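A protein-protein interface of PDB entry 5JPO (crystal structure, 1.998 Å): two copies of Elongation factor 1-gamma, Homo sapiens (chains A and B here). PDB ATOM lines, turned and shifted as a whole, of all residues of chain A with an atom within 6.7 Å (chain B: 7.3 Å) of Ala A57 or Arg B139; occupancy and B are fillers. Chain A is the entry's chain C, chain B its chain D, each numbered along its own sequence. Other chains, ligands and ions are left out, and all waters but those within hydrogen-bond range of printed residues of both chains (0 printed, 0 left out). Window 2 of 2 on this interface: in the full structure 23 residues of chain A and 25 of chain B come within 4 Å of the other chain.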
ATOM      1  N   ASN A  46     -14.833 -17.998 -39.558  1.00  0.00           N
ATOM      2  CA  ASN A  46     -15.590 -17.782 -38.331  1.00  0.00           C
ATOM      3  C   ASN A  46     -15.155 -16.476 -37.667  1.00  0.00           C
ATOM      4  O   ASN A  46     -15.206 -16.338 -36.447  1.00  0.00           O
ATOM      5  CB  ASN A  46     -15.448 -18.979 -37.376  1.00  0.00           C
ATOM      6  CG  ASN A  46     -14.084 -19.058 -36.699  1.00  0.00           C
ATOM      7  OD1 ASN A  46     -13.100 -18.486 -37.164  1.00  0.00           O
ATOM      8  ND2 ASN A  46     -14.027 -19.786 -35.590  1.00  0.00           N
ATOM      9  N   PHE A  51     -20.355 -14.034 -41.188  1.00  0.00           N
ATOM     10  CA  PHE A  51     -20.455 -15.148 -40.236  1.00  0.00           C
ATOM     11  C   PHE A  51     -20.897 -14.634 -38.867  1.00  0.00           C
ATOM     12  O   PHE A  51     -21.815 -15.181 -38.242  1.00  0.00           O
ATOM     13  CB  PHE A  51     -19.120 -15.883 -40.118  1.00  0.00           C
ATOM     14  CG  PHE A  51     -19.189 -17.164 -39.316  1.00  0.00           C
ATOM     15  CD1 PHE A  51     -19.387 -18.383 -39.944  1.00  0.00           C
ATOM     16  CD2 PHE A  51     -19.049 -17.147 -37.935  1.00  0.00           C
ATOM     17  CE1 PHE A  51     -19.447 -19.569 -39.209  1.00  0.00           C
ATOM     18  CE2 PHE A  51     -19.105 -18.322 -37.196  1.00  0.00           C
ATOM     19  CZ  PHE A  51     -19.304 -19.536 -37.835  1.00  0.00           C
ATOM     20  N   LEU A  52     -20.254 -13.560 -38.418  1.00  0.00           N
ATOM     21  CA  LEU A  52     -20.564 -12.983 -37.120  1.00  0.00           C
ATOM     22  C   LEU A  52     -21.965 -12.377 -37.141  1.00  0.00           C
ATOM     23  O   LEU A  52     -22.669 -12.371 -36.130  1.00  0.00           O
ATOM     24  CB  LEU A  52     -19.498 -11.954 -36.745  1.00  0.00           C
ATOM     25  CG  LEU A  52     -18.098 -12.593 -36.802  1.00  0.00           C
ATOM     26  CD1 LEU A  52     -16.997 -11.550 -36.894  1.00  0.00           C
ATOM     27  CD2 LEU A  52     -17.851 -13.530 -35.619  1.00  0.00           C
ATOM     28  N   LYS A  54     -24.547 -13.695 -38.742  1.00  0.00           N
ATOM     29  CA  LYS A  54     -25.430 -14.835 -38.485  1.00  0.00           C
ATOM     30  C   LYS A  54     -25.141 -15.492 -37.136  1.00  0.00           C
ATOM     31  O   LYS A  54     -26.059 -15.879 -36.418  1.00  0.00           O
ATOM     32  CB  LYS A  54     -25.290 -15.894 -39.578  1.00  0.00           C
ATOM     33  CG  LYS A  54     -25.471 -15.413 -40.997  1.00  0.00           C
ATOM     34  CD  LYS A  54     -24.506 -16.171 -41.891  1.00  0.00           C
ATOM     35  CE  LYS A  54     -25.032 -16.381 -43.302  1.00  0.00           C
ATOM     36  NZ  LYS A  54     -24.059 -17.213 -44.073  1.00  0.00           N
ATOM     37  N   PHE A  55     -23.853 -15.631 -36.824  1.00  0.00           N
ATOM     38  CA  PHE A  55     -23.404 -16.326 -35.626  1.00  0.00           C
ATOM     39  C   PHE A  55     -22.471 -15.426 -34.813  1.00  0.00           C
ATOM     40  O   PHE A  55     -21.241 -15.538 -34.906  1.00  0.00           O
ATOM     41  CB  PHE A  55     -22.695 -17.636 -35.998  1.00  0.00           C
ATOM     42  CG  PHE A  55     -23.388 -18.418 -37.084  1.00  0.00           C
ATOM     43  CD1 PHE A  55     -24.639 -18.977 -36.869  1.00  0.00           C
ATOM     44  CD2 PHE A  55     -22.774 -18.608 -38.318  1.00  0.00           C
ATOM     45  CE1 PHE A  55     -25.272 -19.714 -37.874  1.00  0.00           C
ATOM     46  CE2 PHE A  55     -23.402 -19.339 -39.325  1.00  0.00           C
ATOM     47  CZ  PHE A  55     -24.652 -19.886 -39.102  1.00  0.00           C
ATOM     48  N   PRO A  56     -23.064 -14.536 -34.001  1.00  0.00           N
ATOM     49  CA  PRO A  56     -22.362 -13.475 -33.260  1.00  0.00           C
ATOM     50  C   PRO A  56     -21.171 -13.961 -32.437  1.00  0.00           C
ATOM     51  O   PRO A  56     -20.141 -13.286 -32.409  1.00  0.00           O
ATOM     52  CB  PRO A  56     -23.454 -12.901 -32.341  1.00  0.00           C
ATOM     53  CG  PRO A  56     -24.604 -13.874 -32.400  1.00  0.00           C
ATOM     54  CD  PRO A  56     -24.515 -14.530 -33.740  1.00  0.00           C
ATOM     55  N   ALA A  57     -21.306 -15.116 -31.792  1.00  0.00           N
ATOM     56  CA  ALA A  57     -20.265 -15.626 -30.909  1.00  0.00           C
ATOM     57  C   ALA A  57     -19.031 -16.133 -31.659  1.00  0.00           C
ATOM     58  O   ALA A  57     -17.973 -16.342 -31.063  1.00  0.00           O
ATOM     59  CB  ALA A  57     -20.830 -16.729 -30.028  1.00  0.00           C
ATOM     60  N   GLY A  58     -19.170 -16.339 -32.964  1.00  0.00           N
ATOM     61  CA  GLY A  58     -18.051 -16.776 -33.771  1.00  0.00           C
ATOM     62  C   GLY A  58     -17.565 -18.164 -33.392  1.00  0.00           C
ATOM     63  O   GLY A  58     -16.373 -18.449 -33.494  1.00  0.00           O
ATOM     64  N   LYS A  59     -18.483 -19.022 -32.951  1.00  0.00           N
ATOM     65  CA  LYS A  59     -18.139 -20.397 -32.593  1.00  0.00           C
ATOM     66  C   LYS A  59     -18.642 -21.357 -33.647  1.00  0.00           C
ATOM     67  O   LYS A  59     -19.638 -21.087 -34.307  1.00  0.00           O
ATOM     68  CB  LYS A  59     -18.738 -20.781 -31.236  1.00  0.00           C
ATOM     69  CG  LYS A  59     -18.336 -19.878 -30.089  1.00  0.00           C
ATOM     70  CD  LYS A  59     -19.240 -20.085 -28.887  1.00  0.00           C
ATOM     71  CE  LYS A  59     -18.956 -21.409 -28.190  1.00  0.00           C
ATOM     72  NZ  LYS A  59     -19.713 -21.497 -26.902  1.00  0.00           N
ATOM     73  N   PHE A  72     -26.528 -21.363 -33.057  1.00  0.00           N
ATOM     74  CA  PHE A  72     -25.219 -21.883 -32.671  1.00  0.00           C
ATOM     75  C   PHE A  72     -25.287 -22.572 -31.302  1.00  0.00           C
ATOM     76  O   PHE A  72     -26.352 -22.597 -30.674  1.00  0.00           O
ATOM     77  CB  PHE A  72     -24.157 -20.777 -32.678  1.00  0.00           C
ATOM     78  CG  PHE A  72     -24.460 -19.619 -31.755  1.00  0.00           C
ATOM     79  CD1 PHE A  72     -23.849 -19.529 -30.513  1.00  0.00           C
ATOM     80  CD2 PHE A  72     -25.355 -18.627 -32.133  1.00  0.00           C
ATOM     81  CE1 PHE A  72     -24.126 -18.470 -29.662  1.00  0.00           C
ATOM     82  CE2 PHE A  72     -25.638 -17.565 -31.288  1.00  0.00           C
ATOM     83  CZ  PHE A  72     -25.022 -17.491 -30.047  1.00  0.00           C
ATOM     84  N   GLU A  73     -24.146 -23.106 -30.865  1.00  0.00           N
ATOM     85  CA  GLU A  73     -24.015 -24.041 -29.733  1.00  0.00           C
ATOM     86  C   GLU A  73     -24.415 -25.441 -30.199  1.00  0.00           C
ATOM     87  O   GLU A  73     -25.508 -25.635 -30.708  1.00  0.00           O
ATOM     88  CB  GLU A  73     -24.858 -23.629 -28.509  1.00  0.00           C
ATOM     89  CG  GLU A  73     -24.451 -22.309 -27.856  1.00  0.00           C
ATOM     90  CD  GLU A  73     -23.053 -22.371 -27.258  1.00  0.00           C
ATOM     91  OE1 GLU A  73     -22.662 -23.443 -26.731  1.00  0.00           O
ATOM     92  OE2 GLU A  73     -22.337 -21.354 -27.329  1.00  0.00           O
ATOM     93  N   TRP B 100     -28.812 -19.977 -25.863  1.00  0.00           N
ATOM     94  CA  TRP B 100     -28.380 -18.983 -24.871  1.00  0.00           C
ATOM     95  C   TRP B 100     -28.066 -19.626 -23.526  1.00  0.00           C
ATOM     96  O   TRP B 100     -27.190 -19.160 -22.782  1.00  0.00           O
ATOM     97  CB  TRP B 100     -29.444 -17.885 -24.705  1.00  0.00           C
ATOM     98  CG  TRP B 100     -29.514 -16.998 -25.929  1.00  0.00           C
ATOM     99  CD1 TRP B 100     -30.520 -16.935 -26.856  1.00  0.00           C
ATOM    100  CD2 TRP B 100     -28.505 -16.081 -26.365  1.00  0.00           C
ATOM    101  NE1 TRP B 100     -30.202 -16.014 -27.841  1.00  0.00           N
ATOM    102  CE2 TRP B 100     -28.963 -15.481 -27.562  1.00  0.00           C
ATOM    103  CE3 TRP B 100     -27.247 -15.710 -25.871  1.00  0.00           C
ATOM    104  CZ2 TRP B 100     -28.214 -14.544 -28.268  1.00  0.00           C
ATOM    105  CZ3 TRP B 100     -26.500 -14.773 -26.574  1.00  0.00           C
ATOM    106  CH2 TRP B 100     -26.990 -14.197 -27.756  1.00  0.00           C
ATOM    107  N   PHE B 103     -24.717 -21.141 -24.108  1.00  0.00           N
ATOM    108  CA  PHE B 103     -23.739 -20.053 -24.203  1.00  0.00           C
ATOM    109  C   PHE B 103     -23.412 -19.509 -22.805  1.00  0.00           C
ATOM    110  O   PHE B 103     -22.236 -19.336 -22.451  1.00  0.00           O
ATOM    111  CB  PHE B 103     -24.258 -18.937 -25.122  1.00  0.00           C
ATOM    112  CG  PHE B 103     -23.326 -17.768 -25.234  1.00  0.00           C
ATOM    113  CD1 PHE B 103     -22.184 -17.850 -26.017  1.00  0.00           C
ATOM    114  CD2 PHE B 103     -23.579 -16.594 -24.542  1.00  0.00           C
ATOM    115  CE1 PHE B 103     -21.312 -16.782 -26.114  1.00  0.00           C
ATOM    116  CE2 PHE B 103     -22.710 -15.515 -24.640  1.00  0.00           C
ATOM    117  CZ  PHE B 103     -21.567 -15.621 -25.427  1.00  0.00           C
ATOM    118  N   ASP B 107     -19.587 -19.943 -21.823  1.00  0.00           N
ATOM    119  CA  ASP B 107     -18.825 -18.716 -22.043  1.00  0.00           C
ATOM    120  C   ASP B 107     -18.956 -17.652 -20.955  1.00  0.00           C
ATOM    121  O   ASP B 107     -18.056 -16.848 -20.786  1.00  0.00           O
ATOM    122  CB  ASP B 107     -19.222 -18.094 -23.393  1.00  0.00           C
ATOM    123  CG  ASP B 107     -18.656 -18.868 -24.570  1.00  0.00           C
ATOM    124  OD1 ASP B 107     -18.775 -20.113 -24.579  1.00  0.00           O
ATOM    125  OD2 ASP B 107     -18.066 -18.245 -25.474  1.00  0.00           O
ATOM    126  N   ILE B 108     -20.070 -17.617 -20.235  1.00  0.00           N
ATOM    127  CA  ILE B 108     -20.256 -16.552 -19.247  1.00  0.00           C
ATOM    128  C   ILE B 108     -19.899 -16.995 -17.827  1.00  0.00           C
ATOM    129  O   ILE B 108     -19.211 -16.273 -17.105  1.00  0.00           O
ATOM    130  CB  ILE B 108     -21.708 -16.012 -19.252  1.00  0.00           C
ATOM    131  CG1 ILE B 108     -22.162 -15.669 -20.678  1.00  0.00           C
ATOM    132  CG2 ILE B 108     -21.808 -14.780 -18.384  1.00  0.00           C
ATOM    133  CD1 ILE B 108     -23.547 -14.991 -20.734  1.00  0.00           C
ATOM    134  N   ALA B 133     -10.371 -12.289 -17.028  1.00  0.00           N
ATOM    135  CA  ALA B 133     -11.817 -12.456 -16.939  1.00  0.00           C
ATOM    136  C   ALA B 133     -12.543 -11.175 -17.352  1.00  0.00           C
ATOM    137  O   ALA B 133     -13.591 -11.220 -18.009  1.00  0.00           O
ATOM    138  CB  ALA B 133     -12.212 -12.868 -15.529  1.00  0.00           C
ATOM    139  N   LYS B 134     -11.984 -10.027 -16.969  1.00  0.00           N
ATOM    140  CA  LYS B 134     -12.595  -8.736 -17.280  1.00  0.00           C
ATOM    141  C   LYS B 134     -12.684  -8.536 -18.798  1.00  0.00           C
ATOM    142  O   LYS B 134     -13.690  -8.050 -19.328  1.00  0.00           O
ATOM    143  CB  LYS B 134     -11.803  -7.598 -16.609  1.00  0.00           C
ATOM    144  CG  LYS B 134     -12.361  -6.211 -16.824  1.00  0.00           C
ATOM    145  CD  LYS B 134     -11.687  -5.181 -15.899  1.00  0.00           C
ATOM    146  CE  LYS B 134     -12.172  -3.759 -16.207  1.00  0.00           C
ATOM    147  NZ  LYS B 134     -11.611  -2.754 -15.254  1.00  0.00           N
ATOM    148  N   GLU B 135     -11.641  -8.943 -19.509  1.00  0.00           N
ATOM    149  CA  GLU B 135     -11.664  -8.856 -20.966  1.00  0.00           C
ATOM    150  C   GLU B 135     -12.688  -9.820 -21.584  1.00  0.00           C
ATOM    151  O   GLU B 135     -13.378  -9.451 -22.533  1.00  0.00           O
ATOM    152  CB  GLU B 135     -10.268  -9.119 -21.538  1.00  0.00           C
ATOM    153  CG  GLU B 135     -10.151  -8.874 -23.029  1.00  0.00           C
ATOM    154  CD  GLU B 135     -10.559  -7.455 -23.450  1.00  0.00           C
ATOM    155  OE1 GLU B 135     -10.393  -6.495 -22.650  1.00  0.00           O
ATOM    156  OE2 GLU B 135     -11.036  -7.307 -24.598  1.00  0.00           O
ATOM    157  N   GLU B 136     -12.794 -11.046 -21.062  1.00  0.00           N
ATOM    158  CA  GLU B 136     -13.810 -11.973 -21.575  1.00  0.00           C
ATOM    159  C   GLU B 136     -15.221 -11.425 -21.342  1.00  0.00           C
ATOM    160  O   GLU B 136     -16.094 -11.548 -22.195  1.00  0.00           O
ATOM    161  CB  GLU B 136     -13.701 -13.359 -20.922  1.00  0.00           C
ATOM    162  CG  GLU B 136     -12.605 -14.243 -21.463  1.00  0.00           C
ATOM    163  CD  GLU B 136     -12.521 -15.580 -20.728  1.00  0.00           C
ATOM    164  OE1 GLU B 136     -11.666 -15.715 -19.831  1.00  0.00           O
ATOM    165  OE2 GLU B 136     -13.320 -16.492 -21.035  1.00  0.00           O
ATOM    166  N   VAL B 137     -15.450 -10.852 -20.168  1.00  0.00           N
ATOM    167  CA  VAL B 137     -16.763 -10.316 -19.848  1.00  0.00           C
ATOM    168  C   VAL B 137     -17.067  -9.117 -20.754  1.00  0.00           C
ATOM    169  O   VAL B 137     -18.194  -8.954 -21.236  1.00  0.00           O
ATOM    170  CB  VAL B 137     -16.861  -9.911 -18.352  1.00  0.00           C
ATOM    171  CG1 VAL B 137     -18.073  -8.986 -18.116  1.00  0.00           C
ATOM    172  CG2 VAL B 137     -16.913 -11.163 -17.470  1.00  0.00           C
ATOM    173  N   ARG B 138     -16.053  -8.290 -21.001  1.00  0.00           N
ATOM    174  CA  ARG B 138     -16.223  -7.163 -21.908  1.00  0.00           C
ATOM    175  C   ARG B 138     -16.691  -7.653 -23.268  1.00  0.00           C
ATOM    176  O   ARG B 138     -17.606  -7.082 -23.850  1.00  0.00           O
ATOM    177  CB  ARG B 138     -14.926  -6.359 -22.048  1.00  0.00           C
ATOM    178  CG  ARG B 138     -15.164  -4.886 -22.309  1.00  0.00           C
ATOM    179  CD  ARG B 138     -13.856  -4.123 -22.436  1.00  0.00           C
ATOM    180  NE  ARG B 138     -13.042  -4.672 -23.512  1.00  0.00           N
ATOM    181  CZ  ARG B 138     -13.200  -4.371 -24.799  1.00  0.00           C
ATOM    182  NH1 ARG B 138     -14.142  -3.512 -25.175  1.00  0.00           N
ATOM    183  NH2 ARG B 138     -12.414  -4.931 -25.713  1.00  0.00           N
ATOM    184  N   ARG B 139     -16.087  -8.733 -23.758  1.00  0.00           N
ATOM    185  CA  ARG B 139     -16.489  -9.321 -25.036  1.00  0.00           C
ATOM    186  C   ARG B 139     -17.940  -9.832 -25.010  1.00  0.00           C
ATOM    187  O   ARG B 139     -18.704  -9.619 -25.957  1.00  0.00           O
ATOM    188  CB  ARG B 139     -15.544 -10.461 -25.418  1.00  0.00           C
ATOM    189  CG  ARG B 139     -15.699 -10.929 -26.861  1.00  0.00           C
ATOM    190  CD  ARG B 139     -15.074 -12.309 -27.105  1.00  0.00           C
ATOM    191  NE  ARG B 139     -15.695 -13.362 -26.293  1.00  0.00           N
ATOM    192  CZ  ARG B 139     -16.540 -14.279 -26.758  1.00  0.00           C
ATOM    193  NH1 ARG B 139     -16.878 -14.290 -28.046  1.00  0.00           N
ATOM    194  NH2 ARG B 139     -17.044 -15.195 -25.931  1.00  0.00           N
ATOM    195  N   ILE B 140     -18.314 -10.495 -23.921  1.00  0.00           N
ATOM    196  CA  ILE B 140     -19.659 -11.039 -23.756  1.00  0.00           C
ATOM    197  C   ILE B 140     -20.731  -9.951 -23.732  1.00  0.00           C
ATOM    198  O   ILE B 140     -21.744 -10.074 -24.422  1.00  0.00           O
ATOM    199  CB  ILE B 140     -19.780 -11.859 -22.454  1.00  0.00           C
ATOM    200  CG1 ILE B 140     -19.091 -13.215 -22.596  1.00  0.00           C
ATOM    201  CG2 ILE B 140     -21.245 -12.068 -22.075  1.00  0.00           C
ATOM    202  CD1 ILE B 140     -18.788 -13.826 -21.242  1.00  0.00           C
ATOM    203  N   LEU B 141     -20.504  -8.895 -22.950  1.00  0.00           N
ATOM    204  CA  LEU B 141     -21.487  -7.820 -22.826  1.00  0.00           C
ATOM    205  C   LEU B 141     -21.651  -7.115 -24.156  1.00  0.00           C
ATOM    206  O   LEU B 141     -22.728  -6.635 -24.474  1.00  0.00           O
ATOM    207  CB  LEU B 141     -21.077  -6.819 -21.745  1.00  0.00           C
ATOM    208  CG  LEU B 141     -20.966  -7.401 -20.337  1.00  0.00           C
ATOM    209  CD1 LEU B 141     -20.498  -6.346 -19.343  1.00  0.00           C
ATOM    210  CD2 LEU B 141     -22.293  -7.998 -19.902  1.00  0.00           C
ATOM    211  N   GLY B 142     -20.565  -7.046 -24.920  1.00  0.00           N
ATOM    212  CA  GLY B 142     -20.568  -6.395 -26.218  1.00  0.00           C
ATOM    213  C   GLY B 142     -21.362  -7.203 -27.222  1.00  0.00           C
ATOM    214  O   GLY B 142     -22.062  -6.645 -28.074  1.00  0.00           O
ATOM    215  N   LEU B 143     -21.254  -8.527 -27.106  1.00  0.00           N
ATOM    216  CA  LEU B 143     -22.030  -9.465 -27.921  1.00  0.00           C
ATOM    217  C   LEU B 143     -23.527  -9.357 -27.631  1.00  0.00           C
ATOM    218  O   LEU B 143     -24.345  -9.303 -28.553  1.00  0.00           O
ATOM    219  CB  LEU B 143     -21.547 -10.889 -27.677  1.00  0.00           C
ATOM    220  CG  LEU B 143     -22.006 -12.030 -28.590  1.00  0.00           C
ATOM    221  CD1 LEU B 143     -20.980 -13.161 -28.516  1.00  0.00           C
ATOM    222  CD2 LEU B 143     -23.386 -12.543 -28.196  1.00  0.00           C
ATOM    223  N   LEU B 144     -23.883  -9.348 -26.351  1.00  0.00           N
ATOM    224  CA  LEU B 144     -25.272  -9.163 -25.956  1.00  0.00           C
ATOM    225  C   LEU B 144     -25.752  -7.780 -26.402  1.00  0.00           C
ATOM    226  O   LEU B 144     -26.906  -7.621 -26.822  1.00  0.00           O
ATOM    227  CB  LEU B 144     -25.427  -9.331 -24.442  1.00  0.00           C
ATOM    228  CG  LEU B 144     -25.219 -10.763 -23.900  1.00  0.00           C
ATOM    229  CD1 LEU B 144     -25.141 -10.798 -22.379  1.00  0.00           C
ATOM    230  CD2 LEU B 144     -26.324 -11.671 -24.391  1.00  0.00           C
ATOM    231  N   ASP B 145     -24.869  -6.784 -26.318  1.00  0.00           N
ATOM    232  CA  ASP B 145     -25.281  -5.411 -26.605  1.00  0.00           C
ATOM    233  C   ASP B 145     -25.724  -5.255 -28.045  1.00  0.00           C
ATOM    234  O   ASP B 145     -26.752  -4.625 -28.316  1.00  0.00           O
ATOM    235  CB  ASP B 145     -24.157  -4.416 -26.309  1.00  0.00           C
ATOM    236  CG  ASP B 145     -24.659  -2.976 -26.274  1.00  0.00           C
ATOM    237  OD1 ASP B 145     -25.148  -2.557 -25.204  1.00  0.00           O
ATOM    238  OD2 ASP B 145     -24.587  -2.264 -27.303  1.00  0.00           O
ATOM    239  N   PHE B 182     -17.282   1.083 -16.587  1.00  0.00           N
ATOM    240  CA  PHE B 182     -17.130  -0.127 -17.381  1.00  0.00           C
ATOM    241  C   PHE B 182     -18.413  -0.492 -18.130  1.00  0.00           C
ATOM    242  O   PHE B 182     -18.365  -0.818 -19.310  1.00  0.00           O
ATOM    243  CB  PHE B 182     -16.704  -1.295 -16.496  1.00  0.00           C
ATOM    244  CG  PHE B 182     -16.463  -2.572 -17.249  1.00  0.00           C
ATOM    245  CD1 PHE B 182     -15.208  -2.859 -17.766  1.00  0.00           C
ATOM    246  CD2 PHE B 182     -17.481  -3.495 -17.422  1.00  0.00           C
ATOM    247  CE1 PHE B 182     -14.970  -4.045 -18.446  1.00  0.00           C
ATOM    248  CE2 PHE B 182     -17.250  -4.692 -18.115  1.00  0.00           C
ATOM    249  CZ  PHE B 182     -15.995  -4.959 -18.624  1.00  0.00           C
ATOM    250  N   PHE B 186     -22.223  -0.545 -22.623  1.00  0.00           N
ATOM    251  CA  PHE B 186     -23.229  -1.555 -23.007  1.00  0.00           C
ATOM    252  C   PHE B 186     -24.666  -1.167 -22.613  1.00  0.00           C
ATOM    253  O   PHE B 186     -25.334  -1.902 -21.883  1.00  0.00           O
ATOM    254  CB  PHE B 186     -22.863  -2.930 -22.391  1.00  0.00           C
ATOM    255  CG  PHE B 186     -21.379  -3.262 -22.466  1.00  0.00           C
ATOM    256  CD1 PHE B 186     -20.781  -3.635 -23.665  1.00  0.00           C
ATOM    257  CD2 PHE B 186     -20.590  -3.162 -21.338  1.00  0.00           C
ATOM    258  CE1 PHE B 186     -19.420  -3.918 -23.727  1.00  0.00           C
ATOM    259  CE2 PHE B 186     -19.227  -3.435 -21.382  1.00  0.00           C
ATOM    260  CZ  PHE B 186     -18.636  -3.816 -22.580  1.00  0.00           C
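NZ of Lys A59 is in salt-bridge range of OD1 of Asp B107 (2.9 Å).
NZ of Lys A59 is in salt-bridge range of OE2 of Glu A73 (2.7 Å).
The side-chain carboxylate of Asp B107 is in salt-bridge range of the guanidinium group of Arg B139 (3.2 Å).
Pro A56 touches Leu B143 (O to CD1, 3.98 Å).
Ala A57 touches Phe B103.
Arg B139 touches Ala A57 (NH1 to O, 3.8 Å).
Leu B143 touches Ala A57 (CD1 to CA, 3.5 Å).
OE2 of Glu A73 touches CA of Phe B103, 3.7 Å away.
Of the printed residues of chain B, Pro A56 touches Leu B143 (3.98 Å).
Of chain B, only Phe B103 (3.9 Å), Arg B139 (3.8 Å) and Leu B143 (3.5 Å) come within 4 Å of Ala A57.
Of the printed residues of chain B, Lys A59 touches Asp B107 (2.9 Å).
Of the printed residues of chain B, Glu A73 touches Phe B103 (3.7 Å).
Of the printed residues of chain A, Phe B103 touches Ala A57 (3.9 Å) and Glu A73 (3.7 Å).
Val B137 touches none of the printed residues of chain A.
Of chain A, only Ala A57 comes within 4 Å of Arg B139.
Of the printed residues of chain A, Leu B143 touches Pro A56 (3.98 Å) and Ala A57 (3.5 Å).
The nearest residue of chain B that does not touch Ala A57 is Asp B107 (5.5 Å).
The nearest residue of chain A that does not touch Arg B139 is Pro A56 (5.5 Å).
Hydrophobic or aromatic side chains of chain A within 4 Å of the printed part of chain B: Ala A57.
Printed residues of chain B that touch a printed residue of chain A: Phe B103, Asp B107, Arg B139 and Leu B143.
No position is printed for both chains.
Of the 6 pairs that touch across the chains among the printed residues, none has its exchanged pair printed and touching as well.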
